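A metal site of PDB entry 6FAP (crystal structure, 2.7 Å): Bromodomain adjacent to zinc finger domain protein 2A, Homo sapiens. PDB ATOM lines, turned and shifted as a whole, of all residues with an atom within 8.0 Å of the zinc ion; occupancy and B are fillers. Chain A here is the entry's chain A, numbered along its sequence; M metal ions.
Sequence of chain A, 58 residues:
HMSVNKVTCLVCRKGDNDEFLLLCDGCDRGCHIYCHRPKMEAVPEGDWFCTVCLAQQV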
ATOM      1  N   LEU A  10       8.851 -21.711  22.958  1.00  0.00           N
ATOM      2  CA  LEU A  10       7.569 -22.303  22.547  1.00  0.00           C
ATOM      3  C   LEU A  10       7.504 -22.541  21.042  1.00  0.00           C
ATOM      4  O   LEU A  10       6.909 -23.518  20.593  1.00  0.00           O
ATOM      5  CB  LEU A  10       6.405 -21.404  22.966  1.00  0.00           C
ATOM      6  CG  LEU A  10       6.120 -21.292  24.465  1.00  0.00           C
ATOM      7  CD1 LEU A  10       5.226 -20.098  24.759  1.00  0.00           C
ATOM      8  CD2 LEU A  10       5.505 -22.571  24.998  1.00  0.00           C
ATOM      9  N   LEU A  23      11.526 -14.685  29.136  1.00  0.00           N
ATOM     10  CA  LEU A  23      10.920 -15.508  30.171  1.00  0.00           C
ATOM     11  C   LEU A  23       9.594 -14.891  30.572  1.00  0.00           C
ATOM     12  O   LEU A  23       9.521 -13.697  30.900  1.00  0.00           O
ATOM     13  CB  LEU A  23      11.852 -15.591  31.381  1.00  0.00           C
ATOM     14  CG  LEU A  23      13.296 -15.971  31.070  1.00  0.00           C
ATOM     15  CD1 LEU A  23      14.167 -15.879  32.312  1.00  0.00           C
ATOM     16  CD2 LEU A  23      13.365 -17.374  30.470  1.00  0.00           C
ATOM     17  N   CYS A  24       8.533 -15.686  30.516  1.00  0.00           N
ATOM     18  CA  CYS A  24       7.208 -15.234  30.933  1.00  0.00           C
ATOM     19  C   CYS A  24       7.211 -14.942  32.430  1.00  0.00           C
ATOM     20  O   CYS A  24       7.763 -15.713  33.218  1.00  0.00           O
ATOM     21  CB  CYS A  24       6.153 -16.287  30.609  1.00  0.00           C
ATOM     22  SG  CYS A  24       4.479 -15.852  31.115  1.00  0.00           S
ATOM     23  N   ASP A  25       6.605 -13.828  32.811  1.00  0.00           N
ATOM     24  CA  ASP A  25       6.531 -13.443  34.218  1.00  0.00           C
ATOM     25  C   ASP A  25       5.292 -14.012  34.901  1.00  0.00           C
ATOM     26  O   ASP A  25       5.124 -13.873  36.114  1.00  0.00           O
ATOM     27  CB  ASP A  25       6.572 -11.909  34.338  1.00  0.00           C
ATOM     28  CG  ASP A  25       7.799 -11.315  33.674  1.00  0.00           C
ATOM     29  OD1 ASP A  25       8.888 -11.335  34.289  1.00  0.00           O
ATOM     30  OD2 ASP A  25       7.687 -10.855  32.519  1.00  0.00           O
ATOM     31  N   GLY A  26       4.431 -14.655  34.121  1.00  0.00           N
ATOM     32  CA  GLY A  26       3.274 -15.375  34.661  1.00  0.00           C
ATOM     33  C   GLY A  26       3.511 -16.861  34.859  1.00  0.00           C
ATOM     34  O   GLY A  26       2.832 -17.494  35.662  1.00  0.00           O
ATOM     35  N   CYS A  27       4.463 -17.423  34.110  1.00  0.00           N
ATOM     36  CA  CYS A  27       4.769 -18.853  34.203  1.00  0.00           C
ATOM     37  C   CYS A  27       6.246 -19.100  33.910  1.00  0.00           C
ATOM     38  O   CYS A  27       7.064 -18.202  34.074  1.00  0.00           O
ATOM     39  CB  CYS A  27       3.848 -19.636  33.263  1.00  0.00           C
ATOM     40  SG  CYS A  27       4.257 -19.490  31.508  1.00  0.00           S
ATOM     41  N   ASP A  28       6.599 -20.327  33.505  1.00  0.00           N
ATOM     42  CA  ASP A  28       8.007 -20.692  33.304  1.00  0.00           C
ATOM     43  C   ASP A  28       8.329 -21.019  31.845  1.00  0.00           C
ATOM     44  O   ASP A  28       9.315 -21.697  31.545  1.00  0.00           O
ATOM     45  CB  ASP A  28       8.395 -21.866  34.217  1.00  0.00           C
ATOM     46  CG  ASP A  28       7.487 -23.074  34.055  1.00  0.00           C
ATOM     47  OD1 ASP A  28       6.507 -23.000  33.288  1.00  0.00           O
ATOM     48  OD2 ASP A  28       7.756 -24.107  34.716  1.00  0.00           O
ATOM     49  N   ARG A  29       7.523 -20.474  30.931  1.00  0.00           N
ATOM     50  CA  ARG A  29       7.733 -20.679  29.497  1.00  0.00           C
ATOM     51  C   ARG A  29       8.611 -19.561  28.949  1.00  0.00           C
ATOM     52  O   ARG A  29       8.924 -18.605  29.665  1.00  0.00           O
ATOM     53  CB  ARG A  29       6.390 -20.689  28.757  1.00  0.00           C
ATOM     54  CG  ARG A  29       5.546 -21.941  29.002  1.00  0.00           C
ATOM     55  CD  ARG A  29       4.108 -21.720  28.580  1.00  0.00           C
ATOM     56  NE  ARG A  29       3.272 -22.895  28.821  1.00  0.00           N
ATOM     57  CZ  ARG A  29       2.505 -23.086  29.903  1.00  0.00           C
ATOM     58  NH1 ARG A  29       2.458 -22.173  30.879  1.00  0.00           N
ATOM     59  NH2 ARG A  29       1.783 -24.186  30.018  1.00  0.00           N
ATOM     60  N   GLY A  30       9.028 -19.675  27.689  1.00  0.00           N
ATOM     61  CA  GLY A  30       9.919 -18.675  27.091  1.00  0.00           C
ATOM     62  C   GLY A  30       9.793 -18.545  25.587  1.00  0.00           C
ATOM     63  O   GLY A  30       9.116 -19.340  24.930  1.00  0.00           O
ATOM     64  N   TRP A  48       6.761  -9.321  30.495  1.00  0.00           N
ATOM     65  CA  TRP A  48       6.226  -9.919  29.274  1.00  0.00           C
ATOM     66  C   TRP A  48       5.446 -11.191  29.603  1.00  0.00           C
ATOM     67  O   TRP A  48       5.862 -11.989  30.452  1.00  0.00           O
ATOM     68  CB  TRP A  48       7.346 -10.228  28.295  1.00  0.00           C
ATOM     69  CG  TRP A  48       6.887 -10.993  27.098  1.00  0.00           C
ATOM     70  CD1 TRP A  48       6.215 -10.485  26.027  1.00  0.00           C
ATOM     71  CD2 TRP A  48       7.020 -12.395  26.870  1.00  0.00           C
ATOM     72  NE1 TRP A  48       5.945 -11.490  25.128  1.00  0.00           N
ATOM     73  CE2 TRP A  48       6.434 -12.676  25.621  1.00  0.00           C
ATOM     74  CE3 TRP A  48       7.599 -13.447  27.591  1.00  0.00           C
ATOM     75  CZ2 TRP A  48       6.388 -13.963  25.083  1.00  0.00           C
ATOM     76  CZ3 TRP A  48       7.565 -14.727  27.053  1.00  0.00           C
ATOM     77  CH2 TRP A  48       6.961 -14.973  25.815  1.00  0.00           C
ATOM     78  N   PHE A  49       4.328 -11.395  28.902  1.00  0.00           N
ATOM     79  CA  PHE A  49       3.480 -12.548  29.129  1.00  0.00           C
ATOM     80  C   PHE A  49       3.338 -13.387  27.873  1.00  0.00           C
ATOM     81  O   PHE A  49       3.065 -12.874  26.780  1.00  0.00           O
ATOM     82  CB  PHE A  49       2.100 -12.093  29.613  1.00  0.00           C
ATOM     83  CG  PHE A  49       2.122 -11.502  30.993  1.00  0.00           C
ATOM     84  CD1 PHE A  49       2.169 -12.322  32.112  1.00  0.00           C
ATOM     85  CD2 PHE A  49       2.111 -10.121  31.168  1.00  0.00           C
ATOM     86  CE1 PHE A  49       2.198 -11.781  33.382  1.00  0.00           C
ATOM     87  CE2 PHE A  49       2.138  -9.576  32.446  1.00  0.00           C
ATOM     88  CZ  PHE A  49       2.179 -10.403  33.545  1.00  0.00           C
ATOM     89  N   CYS A  50       3.505 -14.702  28.035  1.00  0.00           N
ATOM     90  CA  CYS A  50       3.323 -15.646  26.951  1.00  0.00           C
ATOM     91  C   CYS A  50       1.833 -15.785  26.612  1.00  0.00           C
ATOM     92  O   CYS A  50       0.971 -15.375  27.381  1.00  0.00           O
ATOM     93  CB  CYS A  50       3.875 -17.017  27.337  1.00  0.00           C
ATOM     94  SG  CYS A  50       2.735 -18.019  28.304  1.00  0.00           S
ATOM     95  N   THR A  51       1.555 -16.420  25.471  1.00  0.00           N
ATOM     96  CA  THR A  51       0.192 -16.539  24.967  1.00  0.00           C
ATOM     97  C   THR A  51      -0.696 -17.434  25.835  1.00  0.00           C
ATOM     98  O   THR A  51      -1.922 -17.274  25.852  1.00  0.00           O
ATOM     99  CB  THR A  51       0.183 -17.070  23.524  1.00  0.00           C
ATOM    100  OG1 THR A  51       1.009 -18.243  23.434  1.00  0.00           O
ATOM    101  CG2 THR A  51       0.712 -16.008  22.577  1.00  0.00           C
ATOM    102  N   VAL A  52      -0.081 -18.356  26.566  1.00  0.00           N
ATOM    103  CA  VAL A  52      -0.829 -19.223  27.486  1.00  0.00           C
ATOM    104  C   VAL A  52      -1.363 -18.420  28.669  1.00  0.00           C
ATOM    105  O   VAL A  52      -2.499 -18.603  29.083  1.00  0.00           O
ATOM    106  CB  VAL A  52       0.034 -20.402  27.996  1.00  0.00           C
ATOM    107  CG1 VAL A  52      -0.817 -21.352  28.820  1.00  0.00           C
ATOM    108  CG2 VAL A  52       0.685 -21.138  26.828  1.00  0.00           C
ATOM    109  N   CYS A  53      -0.542 -17.500  29.179  1.00  0.00           N
ATOM    110  CA  CYS A  53      -0.959 -16.606  30.274  1.00  0.00           C
ATOM    111  C   CYS A  53      -1.946 -15.523  29.808  1.00  0.00           C
ATOM    112  O   CYS A  53      -2.783 -15.068  30.594  1.00  0.00           O
ATOM    113  CB  CYS A  53       0.261 -15.940  30.908  1.00  0.00           C
ATOM    114  SG  CYS A  53       1.272 -17.072  31.889  1.00  0.00           S
ATOM    115  N   LEU A  54      -1.812 -15.079  28.559  1.00  0.00           N
ATOM    116  CA  LEU A  54      -2.766 -14.125  27.984  1.00  0.00           C
ATOM    117  C   LEU A  54      -4.173 -14.716  27.867  1.00  0.00           C
ATOM    118  O   LEU A  54      -5.160 -13.980  27.928  1.00  0.00           O
ATOM    119  CB  LEU A  54      -2.289 -13.642  26.612  1.00  0.00           C
ATOM    120  CG  LEU A  54      -1.080 -12.694  26.589  1.00  0.00           C
ATOM    121  CD1 LEU A  54      -0.623 -12.465  25.148  1.00  0.00           C
ATOM    122  CD2 LEU A  54      -1.396 -11.365  27.261  1.00  0.00           C
ATOM    123  N   GLN A  56      -5.482 -16.571  30.115  1.00  0.00           N
ATOM    124  CA  GLN A  56      -6.028 -16.537  31.478  1.00  0.00           C
ATOM    125  C   GLN A  56      -6.551 -15.158  31.878  1.00  0.00           C
ATOM    126  O   GLN A  56      -7.222 -15.008  32.897  1.00  0.00           O
ATOM    127  CB  GLN A  56      -4.972 -16.987  32.505  1.00  0.00           C
ATOM    128  CG  GLN A  56      -4.197 -18.250  32.138  1.00  0.00           C
ATOM    129  CD  GLN A  56      -5.083 -19.437  31.833  1.00  0.00           C
ATOM    130  OE1 GLN A  56      -4.864 -20.161  30.856  1.00  0.00           O
ATOM    131  NE2 GLN A  56      -6.087 -19.669  32.672  1.00  0.00           N
HETATM  132 ZN    ZN M   1       3.122 -17.674  30.591  1.00  0.00          ZN
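SG of Cys 27 sits close to NH1 of Arg 29 (3.3 Å). The backbone NH (N) of Gly 26 lies close to the side-chain sulfur (SG) of Cys 24, at 3.2 Å. N of Cys 24 sits at hydrogen-bond distance from O of Arg 29 (3.1 Å). The side-chain sulfur of Cys 50 lies close to the backbone NH of Val 52 (3.3 Å).
Of the 17 residues printed, 4 come within 4 Å of the zinc ion. The nearest printed residue that does not touch the zinc ion is Gly 26 (4.4 Å).
The zinc ion is bound by SG of Cys 27 (2.3 Å), SG of Cys 24 (2.3 Å), SG of Cys 53 (2.3 Å) and SG of Cys 50 (2.3 Å).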
